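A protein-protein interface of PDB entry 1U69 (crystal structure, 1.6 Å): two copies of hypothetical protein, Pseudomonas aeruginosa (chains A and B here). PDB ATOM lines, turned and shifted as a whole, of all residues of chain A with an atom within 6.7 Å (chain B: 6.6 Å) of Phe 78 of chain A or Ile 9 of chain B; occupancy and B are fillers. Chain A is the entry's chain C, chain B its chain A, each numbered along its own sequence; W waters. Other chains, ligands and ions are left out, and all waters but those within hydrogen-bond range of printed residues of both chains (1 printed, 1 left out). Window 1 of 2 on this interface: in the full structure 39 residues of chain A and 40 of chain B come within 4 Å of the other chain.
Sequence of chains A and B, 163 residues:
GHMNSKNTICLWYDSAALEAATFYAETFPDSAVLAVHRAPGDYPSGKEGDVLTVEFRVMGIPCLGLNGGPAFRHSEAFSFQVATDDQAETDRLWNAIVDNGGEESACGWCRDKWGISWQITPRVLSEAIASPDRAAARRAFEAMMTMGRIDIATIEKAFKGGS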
ATOM      1  N   ILE A   9      -0.688  24.485 -20.215  1.00  0.00           N
ATOM      2  CA  ILE A   9      -1.188  25.753 -19.692  1.00  0.00           C
ATOM      3  C   ILE A   9      -0.011  26.683 -19.413  1.00  0.00           C
ATOM      4  O   ILE A   9       0.832  26.374 -18.566  1.00  0.00           O
ATOM      5  CB  ILE A   9      -1.997  25.506 -18.389  1.00  0.00           C
ATOM      6  CG1 ILE A   9      -3.264  24.719 -18.687  1.00  0.00           C
ATOM      7  CG2 ILE A   9      -2.270  26.799 -17.624  1.00  0.00           C
ATOM      8  CD1 ILE A   9      -4.244  25.372 -19.643  1.00  0.00           C
ATOM      9  N   LEU A  11       1.362  30.268 -18.131  1.00  0.00           N
ATOM     10  CA  LEU A  11       1.043  31.360 -17.216  1.00  0.00           C
ATOM     11  C   LEU A  11       2.193  32.353 -17.121  1.00  0.00           C
ATOM     12  O   LEU A  11       3.356  31.967 -16.970  1.00  0.00           O
ATOM     13  CB  LEU A  11       0.697  30.794 -15.854  1.00  0.00           C
ATOM     14  CG  LEU A  11      -0.545  29.892 -15.825  1.00  0.00           C
ATOM     15  CD1 LEU A  11      -0.565  29.110 -14.521  1.00  0.00           C
ATOM     16  CD2 LEU A  11      -1.822  30.688 -16.013  1.00  0.00           C
ATOM     17  N   ILE A  61      -2.262  18.758 -14.307  1.00  0.00           N
ATOM     18  CA  ILE A  61      -2.249  19.660 -15.463  1.00  0.00           C
ATOM     19  C   ILE A  61      -0.815  20.104 -15.762  1.00  0.00           C
ATOM     20  O   ILE A  61      -0.158  20.664 -14.902  1.00  0.00           O
ATOM     21  CB  ILE A  61      -3.104  20.914 -15.196  1.00  0.00           C
ATOM     22  CG1 ILE A  61      -4.557  20.567 -14.841  1.00  0.00           C
ATOM     23  CG2 ILE A  61      -3.055  21.886 -16.381  1.00  0.00           C
ATOM     24  CD1 ILE A  61      -5.299  19.809 -15.886  1.00  0.00           C
ATOM     25  N   HIS A  74      -2.832  39.077 -14.730  1.00  0.00           N
ATOM     26  CA  HIS A  74      -3.889  38.064 -14.626  1.00  0.00           C
ATOM     27  C   HIS A  74      -5.244  38.687 -14.292  1.00  0.00           C
ATOM     28  O   HIS A  74      -5.328  39.768 -13.703  1.00  0.00           O
ATOM     29  CB  HIS A  74      -3.508  36.990 -13.585  1.00  0.00           C
ATOM     30  CG  HIS A  74      -2.382  36.114 -14.037  1.00  0.00           C
ATOM     31  ND1 HIS A  74      -2.543  35.164 -15.016  1.00  0.00           N
ATOM     32  CD2 HIS A  74      -1.072  36.078 -13.692  1.00  0.00           C
ATOM     33  CE1 HIS A  74      -1.387  34.579 -15.260  1.00  0.00           C
ATOM     34  NE2 HIS A  74      -0.478  35.114 -14.472  1.00  0.00           N
ATOM     35  N   SER A  75      -6.299  38.007 -14.713  1.00  0.00           N
ATOM     36  CA  SER A  75      -7.653  38.379 -14.339  1.00  0.00           C
ATOM     37  C   SER A  75      -8.501  37.126 -14.227  1.00  0.00           C
ATOM     38  O   SER A  75      -8.091  36.033 -14.641  1.00  0.00           O
ATOM     39  CB  SER A  75      -8.260  39.316 -15.364  1.00  0.00           C
ATOM     40  OG  SER A  75      -8.798  38.605 -16.455  1.00  0.00           O
ATOM     41  N   GLU A  76      -9.701  37.320 -13.700  1.00  0.00           N
ATOM     42  CA  GLU A  76     -10.650  36.247 -13.464  1.00  0.00           C
ATOM     43  C   GLU A  76     -11.086  35.539 -14.739  1.00  0.00           C
ATOM     44  O   GLU A  76     -11.732  34.508 -14.669  1.00  0.00           O
ATOM     45  CB  GLU A  76     -11.887  36.816 -12.759  1.00  0.00           C
ATOM     46  CG  GLU A  76     -11.651  37.085 -11.281  1.00  0.00           C
ATOM     47  CD  GLU A  76     -11.169  38.491 -10.961  1.00  0.00           C
ATOM     48  OE1 GLU A  76     -10.547  39.165 -11.807  1.00  0.00           O
ATOM     49  OE2 GLU A  76     -11.414  38.952  -9.816  1.00  0.00           O
ATOM     50  N   ALA A  77     -10.720  36.078 -15.898  1.00  0.00           N
ATOM     51  CA  ALA A  77     -11.012  35.437 -17.182  1.00  0.00           C
ATOM     52  C   ALA A  77     -10.474  33.994 -17.242  1.00  0.00           C
ATOM     53  O   ALA A  77     -11.053  33.138 -17.910  1.00  0.00           O
ATOM     54  CB  ALA A  77     -10.438  36.267 -18.325  1.00  0.00           C
ATOM     55  N   PHE A  78      -9.347  33.755 -16.563  1.00  0.00           N
ATOM     56  CA  PHE A  78      -8.798  32.411 -16.361  1.00  0.00           C
ATOM     57  C   PHE A  78      -8.802  32.073 -14.876  1.00  0.00           C
ATOM     58  O   PHE A  78      -8.451  32.901 -14.066  1.00  0.00           O
ATOM     59  CB  PHE A  78      -7.361  32.302 -16.881  1.00  0.00           C
ATOM     60  CG  PHE A  78      -6.631  31.085 -16.325  1.00  0.00           C
ATOM     61  CD1 PHE A  78      -6.917  29.830 -16.819  1.00  0.00           C
ATOM     62  CD2 PHE A  78      -5.733  31.186 -15.271  1.00  0.00           C
ATOM     63  CE1 PHE A  78      -6.289  28.698 -16.298  1.00  0.00           C
ATOM     64  CE2 PHE A  78      -5.118  30.054 -14.745  1.00  0.00           C
ATOM     65  CZ  PHE A  78      -5.392  28.816 -15.261  1.00  0.00           C
ATOM     66  N   SER A  79      -9.177  30.853 -14.539  1.00  0.00           N
ATOM     67  CA  SER A  79      -9.015  30.358 -13.186  1.00  0.00           C
ATOM     68  C   SER A  79      -8.828  28.844 -13.169  1.00  0.00           C
ATOM     69  O   SER A  79      -9.240  28.140 -14.087  1.00  0.00           O
ATOM     70  CB  SER A  79     -10.202  30.760 -12.305  1.00  0.00           C
ATOM     71  OG  SER A  79     -11.420  30.285 -12.857  1.00  0.00           O
ATOM     72  N   PHE A  80      -8.148  28.355 -12.144  1.00  0.00           N
ATOM     73  CA  PHE A  80      -8.107  26.930 -11.861  1.00  0.00           C
ATOM     74  C   PHE A  80      -9.263  26.622 -10.896  1.00  0.00           C
ATOM     75  O   PHE A  80      -9.315  27.210  -9.822  1.00  0.00           O
ATOM     76  CB  PHE A  80      -6.812  26.547 -11.164  1.00  0.00           C
ATOM     77  CG  PHE A  80      -5.589  26.456 -12.050  1.00  0.00           C
ATOM     78  CD1 PHE A  80      -5.525  25.566 -13.114  1.00  0.00           C
ATOM     79  CD2 PHE A  80      -4.460  27.233 -11.756  1.00  0.00           C
ATOM     80  CE1 PHE A  80      -4.343  25.450 -13.870  1.00  0.00           C
ATOM     81  CE2 PHE A  80      -3.293  27.101 -12.501  1.00  0.00           C
ATOM     82  CZ  PHE A  80      -3.250  26.224 -13.560  1.00  0.00           C
ATOM     83  N   GLN A  81     -10.167  25.715 -11.264  1.00  0.00           N
ATOM     84  CA  GLN A  81     -11.248  25.289 -10.384  1.00  0.00           C
ATOM     85  C   GLN A  81     -10.862  23.947  -9.780  1.00  0.00           C
ATOM     86  O   GLN A  81     -10.719  22.952 -10.495  1.00  0.00           O
ATOM     87  CB  GLN A  81     -12.594  25.177 -11.119  1.00  0.00           C
ATOM     88  CG  GLN A  81     -13.728  24.747 -10.181  1.00  0.00           C
ATOM     89  CD  GLN A  81     -15.073  24.721 -10.839  1.00  0.00           C
ATOM     90  OE1 GLN A  81     -15.781  25.733 -10.867  1.00  0.00           O
ATOM     91  NE2 GLN A  81     -15.446  23.572 -11.361  1.00  0.00           N
ATOM     92  N   TRP A 109     -14.191  31.793  -5.032  1.00  0.00           N
ATOM     93  CA  TRP A 109     -13.057  32.338  -5.767  1.00  0.00           C
ATOM     94  C   TRP A 109     -12.087  33.021  -4.808  1.00  0.00           C
ATOM     95  O   TRP A 109     -12.487  33.655  -3.842  1.00  0.00           O
ATOM     96  CB  TRP A 109     -13.513  33.380  -6.796  1.00  0.00           C
ATOM     97  CG  TRP A 109     -14.283  32.850  -7.937  1.00  0.00           C
ATOM     98  CD1 TRP A 109     -15.490  32.198  -7.887  1.00  0.00           C
ATOM     99  CD2 TRP A 109     -13.924  32.928  -9.319  1.00  0.00           C
ATOM    100  NE1 TRP A 109     -15.895  31.861  -9.156  1.00  0.00           N
ATOM    101  CE2 TRP A 109     -14.960  32.309 -10.056  1.00  0.00           C
ATOM    102  CE3 TRP A 109     -12.840  33.476 -10.014  1.00  0.00           C
ATOM    103  CZ2 TRP A 109     -14.928  32.201 -11.447  1.00  0.00           C
ATOM    104  CZ3 TRP A 109     -12.804  33.361 -11.396  1.00  0.00           C
ATOM    105  CH2 TRP A 109     -13.851  32.743 -12.099  1.00  0.00           C
ATOM    106  N   GLY A 115      -1.413  36.874  -8.577  1.00  0.00           N
ATOM    107  CA  GLY A 115      -2.619  37.372  -9.218  1.00  0.00           C
ATOM    108  C   GLY A 115      -3.483  36.344  -9.922  1.00  0.00           C
ATOM    109  O   GLY A 115      -4.477  36.721 -10.559  1.00  0.00           O
ATOM    110  N   ILE A 116      -3.134  35.066  -9.819  1.00  0.00           N
ATOM    111  CA  ILE A 116      -3.879  33.998 -10.493  1.00  0.00           C
ATOM    112  C   ILE A 116      -5.125  33.651  -9.699  1.00  0.00           C
ATOM    113  O   ILE A 116      -5.074  33.511  -8.477  1.00  0.00           O
ATOM    114  CB  ILE A 116      -2.986  32.782 -10.741  1.00  0.00           C
ATOM    115  CG1 ILE A 116      -1.894  33.199 -11.743  1.00  0.00           C
ATOM    116  CG2 ILE A 116      -3.803  31.584 -11.253  1.00  0.00           C
ATOM    117  CD1 ILE A 116      -0.642  32.461 -11.666  1.00  0.00           C
ATOM    118  N   SER A 117      -6.243  33.526 -10.401  1.00  0.00           N
ATOM    119  CA  SER A 117      -7.522  33.182  -9.791  1.00  0.00           C
ATOM    120  C   SER A 117      -7.646  31.676  -9.571  1.00  0.00           C
ATOM    121  O   SER A 117      -7.344  30.879 -10.469  1.00  0.00           O
ATOM    122  CB  SER A 117      -8.702  33.681 -10.641  1.00  0.00           C
ATOM    123  OG  SER A 117      -8.890  35.083 -10.483  1.00  0.00           O
ATOM    124  N   TRP A 118      -8.138  31.316  -8.386  1.00  0.00           N
ATOM    125  CA  TRP A 118      -8.433  29.933  -8.019  1.00  0.00           C
ATOM    126  C   TRP A 118      -9.865  29.867  -7.529  1.00  0.00           C
ATOM    127  O   TRP A 118     -10.342  30.779  -6.859  1.00  0.00           O
ATOM    128  CB  TRP A 118      -7.515  29.460  -6.889  1.00  0.00           C
ATOM    129  CG  TRP A 118      -6.066  29.409  -7.285  1.00  0.00           C
ATOM    130  CD1 TRP A 118      -5.197  30.438  -7.292  1.00  0.00           C
ATOM    131  CD2 TRP A 118      -5.325  28.254  -7.695  1.00  0.00           C
ATOM    132  NE1 TRP A 118      -3.955  30.013  -7.702  1.00  0.00           N
ATOM    133  CE2 TRP A 118      -4.010  28.670  -7.957  1.00  0.00           C
ATOM    134  CE3 TRP A 118      -5.653  26.901  -7.892  1.00  0.00           C
ATOM    135  CZ2 TRP A 118      -3.015  27.802  -8.393  1.00  0.00           C
ATOM    136  CZ3 TRP A 118      -4.648  26.036  -8.328  1.00  0.00           C
ATOM    137  CH2 TRP A 118      -3.368  26.488  -8.585  1.00  0.00           C
ATOM    138  N   GLN A 119     -10.547  28.775  -7.838  1.00  0.00           N
ATOM    139  CA  GLN A 119     -11.836  28.487  -7.235  1.00  0.00           C
ATOM    140  C   GLN A 119     -11.667  27.235  -6.405  1.00  0.00           C
ATOM    141  O   GLN A 119     -11.209  26.217  -6.905  1.00  0.00           O
ATOM    142  CB  GLN A 119     -12.892  28.239  -8.306  1.00  0.00           C
ATOM    143  CG  GLN A 119     -13.195  29.430  -9.178  1.00  0.00           C
ATOM    144  CD  GLN A 119     -14.175  29.049 -10.263  1.00  0.00           C
ATOM    145  OE1 GLN A 119     -15.313  28.612  -9.964  1.00  0.00           O
ATOM    146  NE2 GLN A 119     -13.749  29.152 -11.506  1.00  0.00           N
ATOM    147  N   ASN B   7      -8.654  19.242 -10.963  1.00  0.00           N
ATOM    148  CA  ASN B   7      -8.311  20.616 -11.331  1.00  0.00           C
ATOM    149  C   ASN B   7      -8.761  20.846 -12.768  1.00  0.00           C
ATOM    150  O   ASN B   7      -8.368  20.120 -13.678  1.00  0.00           O
ATOM    151  CB  ASN B   7      -6.794  20.841 -11.179  1.00  0.00           C
ATOM    152  CG  ASN B   7      -6.380  22.290 -11.410  1.00  0.00           C
ATOM    153  OD1 ASN B   7      -7.202  23.191 -11.316  1.00  0.00           O
ATOM    154  ND2 ASN B   7      -5.096  22.517 -11.734  1.00  0.00           N
ATOM    155  N   THR B   8      -9.605  21.847 -12.955  1.00  0.00           N
ATOM    156  CA  THR B   8     -10.229  22.143 -14.248  1.00  0.00           C
ATOM    157  C   THR B   8      -9.885  23.569 -14.656  1.00  0.00           C
ATOM    158  O   THR B   8      -9.922  24.473 -13.830  1.00  0.00           O
ATOM    159  CB  THR B   8     -11.762  21.985 -14.111  1.00  0.00           C
ATOM    160  OG1 THR B   8     -12.079  20.642 -13.694  1.00  0.00           O
ATOM    161  CG2 THR B   8     -12.478  22.178 -15.442  1.00  0.00           C
ATOM    162  N   ILE B   9      -9.535  23.770 -15.920  1.00  0.00           N
ATOM    163  CA  ILE B   9      -9.227  25.099 -16.452  1.00  0.00           C
ATOM    164  C   ILE B   9     -10.555  25.799 -16.729  1.00  0.00           C
ATOM    165  O   ILE B   9     -11.290  25.343 -17.588  1.00  0.00           O
ATOM    166  CB  ILE B   9      -8.376  24.972 -17.747  1.00  0.00           C
ATOM    167  CG1 ILE B   9      -6.928  24.559 -17.449  1.00  0.00           C
ATOM    168  CG2 ILE B   9      -8.319  26.314 -18.523  1.00  0.00           C
ATOM    169  CD1 ILE B   9      -6.723  23.406 -16.533  1.00  0.00           C
ATOM    170  N   CYS B  10     -10.851  26.890 -16.021  1.00  0.00           N
ATOM    171  CA  CYS B  10     -12.109  27.631 -16.172  1.00  0.00           C
ATOM    172  C   CYS B  10     -11.872  28.905 -16.976  1.00  0.00           C
ATOM    173  O   CYS B  10     -11.061  29.731 -16.594  1.00  0.00           O
ATOM    174  CB  CYS B  10     -12.691  27.974 -14.800  1.00  0.00           C
ATOM    175  SG  CYS B  10     -14.323  28.722 -14.856  1.00  0.00           S
ATOM    176  N   LEU B  11     -12.566  29.034 -18.103  1.00  0.00           N
ATOM    177  CA  LEU B  11     -12.395  30.164 -19.002  1.00  0.00           C
ATOM    178  C   LEU B  11     -13.702  30.932 -19.069  1.00  0.00           C
ATOM    179  O   LEU B  11     -14.763  30.333 -19.222  1.00  0.00           O
ATOM    180  CB  LEU B  11     -12.003  29.674 -20.387  1.00  0.00           C
ATOM    181  CG  LEU B  11     -10.625  29.002 -20.422  1.00  0.00           C
ATOM    182  CD1 LEU B  11     -10.462  28.256 -21.724  1.00  0.00           C
ATOM    183  CD2 LEU B  11      -9.532  30.036 -20.221  1.00  0.00           C
ATOM    184  N   TRP B  12     -13.599  32.257 -18.960  1.00  0.00           N
ATOM    185  CA  TRP B  12     -14.748  33.165 -18.887  1.00  0.00           C
ATOM    186  C   TRP B  12     -15.198  33.540 -20.292  1.00  0.00           C
ATOM    187  O   TRP B  12     -14.377  33.898 -21.138  1.00  0.00           O
ATOM    188  CB  TRP B  12     -14.339  34.426 -18.116  1.00  0.00           C
ATOM    189  CG  TRP B  12     -15.444  35.296 -17.605  1.00  0.00           C
ATOM    190  CD1 TRP B  12     -16.237  36.132 -18.332  1.00  0.00           C
ATOM    191  CD2 TRP B  12     -15.838  35.449 -16.244  1.00  0.00           C
ATOM    192  NE1 TRP B  12     -17.111  36.787 -17.501  1.00  0.00           N
ATOM    193  CE2 TRP B  12     -16.889  36.389 -16.213  1.00  0.00           C
ATOM    194  CE3 TRP B  12     -15.411  34.889 -15.043  1.00  0.00           C
ATOM    195  CZ2 TRP B  12     -17.525  36.765 -15.033  1.00  0.00           C
ATOM    196  CZ3 TRP B  12     -16.047  35.263 -13.864  1.00  0.00           C
ATOM    197  CH2 TRP B  12     -17.095  36.186 -13.871  1.00  0.00           C
ATOM    198  N   PHE B  56     -15.751  20.724 -21.116  1.00  0.00           N
ATOM    199  CA  PHE B  56     -15.145  20.248 -22.351  1.00  0.00           C
ATOM    200  C   PHE B  56     -13.705  19.849 -22.114  1.00  0.00           C
ATOM    201  O   PHE B  56     -13.171  20.114 -21.050  1.00  0.00           O
ATOM    202  CB  PHE B  56     -15.289  21.277 -23.486  1.00  0.00           C
ATOM    203  CG  PHE B  56     -14.503  22.573 -23.297  1.00  0.00           C
ATOM    204  CD1 PHE B  56     -13.265  22.753 -23.904  1.00  0.00           C
ATOM    205  CD2 PHE B  56     -15.043  23.636 -22.577  1.00  0.00           C
ATOM    206  CE1 PHE B  56     -12.568  23.958 -23.755  1.00  0.00           C
ATOM    207  CE2 PHE B  56     -14.358  24.837 -22.466  1.00  0.00           C
ATOM    208  CZ  PHE B  56     -13.127  24.985 -23.050  1.00  0.00           C
ATOM    209  N   ILE B  61      -6.654  18.274 -21.574  1.00  0.00           N
ATOM    210  CA  ILE B  61      -6.906  19.270 -20.534  1.00  0.00           C
ATOM    211  C   ILE B  61      -8.405  19.392 -20.254  1.00  0.00           C
ATOM    212  O   ILE B  61      -9.180  19.758 -21.152  1.00  0.00           O
ATOM    213  CB  ILE B  61      -6.358  20.672 -20.944  1.00  0.00           C
ATOM    214  CG1 ILE B  61      -4.866  20.618 -21.273  1.00  0.00           C
ATOM    215  CG2 ILE B  61      -6.613  21.680 -19.845  1.00  0.00           C
ATOM    216  CD1 ILE B  61      -3.996  20.122 -20.180  1.00  0.00           C
ATOM    217  N   PRO B  62      -8.821  19.120 -19.021  1.00  0.00           N
ATOM    218  CA  PRO B  62     -10.222  19.310 -18.636  1.00  0.00           C
ATOM    219  C   PRO B  62     -10.534  20.793 -18.443  1.00  0.00           C
ATOM    220  O   PRO B  62      -9.796  21.477 -17.724  1.00  0.00           O
ATOM    221  CB  PRO B  62     -10.330  18.550 -17.304  1.00  0.00           C
ATOM    222  CG  PRO B  62      -8.942  18.627 -16.716  1.00  0.00           C
ATOM    223  CD  PRO B  62      -8.010  18.600 -17.903  1.00  0.00           C
ATOM    224  N   CYS B  63     -11.593  21.271 -19.086  1.00  0.00           N
ATOM    225  CA  CYS B  63     -11.942  22.683 -19.075  1.00  0.00           C
ATOM    226  C   CYS B  63     -13.400  22.892 -18.738  1.00  0.00           C
ATOM    227  O   CYS B  63     -14.216  21.977 -18.862  1.00  0.00           O
ATOM    228  CB  CYS B  63     -11.653  23.325 -20.425  1.00  0.00           C
ATOM    229  SG  CYS B  63      -9.951  23.253 -20.990  1.00  0.00           S
ATOM    230  N   LEU B  64     -13.698  24.110 -18.287  1.00  0.00           N
ATOM    231  CA  LEU B  64     -15.054  24.572 -18.024  1.00  0.00           C
ATOM    232  C   LEU B  64     -15.172  25.956 -18.660  1.00  0.00           C
ATOM    233  O   LEU B  64     -14.340  26.823 -18.396  1.00  0.00           O
ATOM    234  CB  LEU B  64     -15.287  24.666 -16.509  1.00  0.00           C
ATOM    235  CG  LEU B  64     -16.721  24.893 -16.019  1.00  0.00           C
ATOM    236  CD1 LEU B  64     -17.531  23.609 -16.182  1.00  0.00           C
ATOM    237  CD2 LEU B  64     -16.722  25.365 -14.565  1.00  0.00           C
ATOM    238  N   GLY B  65     -16.178  26.143 -19.516  1.00  0.00           N
ATOM    239  CA  GLY B  65     -16.506  27.454 -20.063  1.00  0.00           C
ATOM    240  C   GLY B  65     -17.621  28.047 -19.216  1.00  0.00           C
ATOM    241  O   GLY B  65     -18.669  27.417 -19.044  1.00  0.00           O
ATOM    242  N   ARG B  73     -12.075  40.329 -19.082  1.00  0.00           N
ATOM    243  CA  ARG B  73     -11.493  40.155 -20.414  1.00  0.00           C
ATOM    244  C   ARG B  73     -10.221  39.322 -20.337  1.00  0.00           C
ATOM    245  O   ARG B  73      -9.475  39.411 -19.360  1.00  0.00           O
ATOM    246  CB  ARG B  73     -11.154  41.519 -21.019  1.00  0.00           C
ATOM    247  CG  ARG B  73     -12.395  42.340 -21.257  1.00  0.00           C
ATOM    248  CD  ARG B  73     -12.199  43.673 -21.966  1.00  0.00           C
ATOM    249  NE  ARG B  73     -13.026  43.834 -23.171  1.00  0.00           N
ATOM    250  CZ  ARG B  73     -14.339  43.561 -23.293  1.00  0.00           C
ATOM    251  NH1 ARG B  73     -15.076  43.082 -22.280  1.00  0.00           N
ATOM    252  NH2 ARG B  73     -14.927  43.767 -24.470  1.00  0.00           N
ATOM    253  N   HIS B  74      -9.988  38.528 -21.375  1.00  0.00           N
ATOM    254  CA  HIS B  74      -8.778  37.691 -21.465  1.00  0.00           C
ATOM    255  C   HIS B  74      -7.538  38.515 -21.825  1.00  0.00           C
ATOM    256  O   HIS B  74      -7.622  39.596 -22.398  1.00  0.00           O
ATOM    257  CB  HIS B  74      -8.963  36.551 -22.498  1.00  0.00           C
ATOM    258  CG  HIS B  74      -9.939  35.515 -22.048  1.00  0.00           C
ATOM    259  ND1 HIS B  74      -9.663  34.629 -21.032  1.00  0.00           N
ATOM    260  CD2 HIS B  74     -11.221  35.276 -22.414  1.00  0.00           C
ATOM    261  CE1 HIS B  74     -10.730  33.886 -20.798  1.00  0.00           C
ATOM    262  NE2 HIS B  74     -11.689  34.261 -21.616  1.00  0.00           N
ATOM    263  N   ALA B  77      -1.658  36.842 -20.261  1.00  0.00           N
ATOM    264  CA  ALA B  77      -1.290  36.281 -18.960  1.00  0.00           C
ATOM    265  C   ALA B  77      -1.574  34.777 -18.913  1.00  0.00           C
ATOM    266  O   ALA B  77      -0.842  34.021 -18.265  1.00  0.00           O
ATOM    267  CB  ALA B  77      -2.018  37.013 -17.834  1.00  0.00           C
ATOM    268  N   PHE B  78      -2.616  34.346 -19.625  1.00  0.00           N
ATOM    269  CA  PHE B  78      -2.905  32.919 -19.811  1.00  0.00           C
ATOM    270  C   PHE B  78      -2.880  32.577 -21.281  1.00  0.00           C
ATOM    271  O   PHE B  78      -3.405  33.337 -22.108  1.00  0.00           O
ATOM    272  CB  PHE B  78      -4.280  32.553 -19.256  1.00  0.00           C
ATOM    273  CG  PHE B  78      -4.790  31.235 -19.761  1.00  0.00           C
ATOM    274  CD1 PHE B  78      -4.406  30.061 -19.169  1.00  0.00           C
ATOM    275  CD2 PHE B  78      -5.637  31.169 -20.856  1.00  0.00           C
ATOM    276  CE1 PHE B  78      -4.877  28.839 -19.654  1.00  0.00           C
ATOM    277  CE2 PHE B  78      -6.074  29.970 -21.353  1.00  0.00           C
ATOM    278  CZ  PHE B  78      -5.704  28.804 -20.756  1.00  0.00           C
ATOM    279  N   PHE B  80      -2.937  28.701 -23.925  1.00  0.00           N
ATOM    280  CA  PHE B  80      -2.729  27.271 -24.202  1.00  0.00           C
ATOM    281  C   PHE B  80      -1.540  27.201 -25.152  1.00  0.00           C
ATOM    282  O   PHE B  80      -1.538  27.886 -26.149  1.00  0.00           O
ATOM    283  CB  PHE B  80      -3.926  26.659 -24.925  1.00  0.00           C
ATOM    284  CG  PHE B  80      -5.143  26.438 -24.078  1.00  0.00           C
ATOM    285  CD1 PHE B  80      -5.157  25.455 -23.093  1.00  0.00           C
ATOM    286  CD2 PHE B  80      -6.316  27.134 -24.337  1.00  0.00           C
ATOM    287  CE1 PHE B  80      -6.306  25.222 -22.347  1.00  0.00           C
ATOM    288  CE2 PHE B  80      -7.469  26.899 -23.594  1.00  0.00           C
ATOM    289  CZ  PHE B  80      -7.463  25.950 -22.609  1.00  0.00           C
HETATM  290  O   HOH W   1     -12.209  20.692 -10.910  1.00  0.00           O
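The side-chain hydroxyl of Ser 75 of chain A sits at hydrogen-bond distance from the backbone carbonyl oxygen of Arg 73 of chain B, at 3.1 Å.
The backbone NH (N) of Trp 12 of chain B is in hydrogen-bond range of the backbone carbonyl oxygen (O) of Ala 77 of chain A, 2.9 Å away.
The side-chain amide nitrogen of Gln 119 of chain A sits at hydrogen-bond distance from the side-chain sulfur of Cys 10 of chain B, 3.4 Å away.
N of Cys 10 of chain B is in hydrogen-bond range of O of Ser 79 of chain A, at 2.8 Å.
O of Thr 8 of chain B is in hydrogen-bond range of N of Gln 81 of chain A (2.9 Å).
The indole nitrogen of Trp 109 of chain A lies within hydrogen-bond range of the side-chain amide oxygen of Gln 119 of chain A.
The side-chain hydroxyl (OG) of Ser 79 of chain A sits at hydrogen-bond distance from the side-chain amide nitrogen (NE2) of Gln 119 of chain A.
OE1 of Gln 81 of chain A sits close to OE1 of Gln 119 of chain A, at 3.1 Å.
N of Leu 11 of chain B lies within hydrogen-bond range of O of Leu 64 of chain B.
N of Gln 119 of chain A is in hydrogen-bond range of O of Phe 80 of chain A (2.8 Å).
O of Ile 9 of chain B is in hydrogen-bond range of N of Leu 64 of chain B (2.8 Å).
CG1 of Ile 9 of chain B touches CD1 of Ile 9 of chain A (3.6 Å).
Phe 78 of chain B touches Ile 9 of chain A.
His 74 of chain A touches Ala 77 of chain B.
O of Ala 77 of chain A touches O of Cys 10 of chain B, 3.7 Å away.
Phe 78 of chain A touches Ile 9 of chain B (CE1 to CG2, 3.8 Å).
Phe 78 of chain B touches Phe 78 of chain A (CD1 to CD1, 3.4 Å).
O of Ser 79 of chain A touches O of Thr 8 of chain B (3.7 Å).
Ile 9 of chain B touches Ser 79 of chain A.
O of Gln 81 of chain A touches CA of Asn 7 of chain B, 3.5 Å away.
Gln 81 of chain A touches Leu 64 of chain B.
Printed residues of chain B within 4 Å of His 74 of chain A: Ala 77 (3.1 Å).
Phe 78 of chain A touches just these residues of chain B: Ile 9, Cys 10 and Phe 78.
Of the printed residues of chain B, Gln 81 of chain A touches Asn 7, Thr 8 and Leu 64.
Ile 9 of chain B touches just these residues of chain A: Ile 9, Ile 61, Phe 78 and Ser 79.
Of the 17 printed residues of chain B, 13 touch a printed residue of chain A.
Hydrophobic or aromatic side chains of chain B that line the printed part of chain A: Ile 9, Trp 12, Pro 62, Leu 64, His 74, Ala 77, Phe 78 and Phe 80.
Ile 9 of chain B touches its own counterpart, Ile 9 of chain A.
Ile 9 of chain A touches Phe 78 of chain B, and with the chains exchanged Phe 78 of chain A touches Ile 9 of chain B.
Ile 9 of chain A touches Phe 80 of chain B, but with the chains exchanged Phe 80 of chain A does not touch Ile 9 of chain B (4.1 Å).
His 74 of chain A touches Ala 77 of chain B, and with the chains exchanged Ala 77 of chain A touches His 74 of chain B.
Of the 28 pairs that touch across the chains among the printed residues, 8 have their exchanged pair printed and touching as well.
Water W1 bridges the backbone carbonyl oxygen of Gln 81 of chain A and the side-chain hydroxyl of Thr 8 of chain B.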
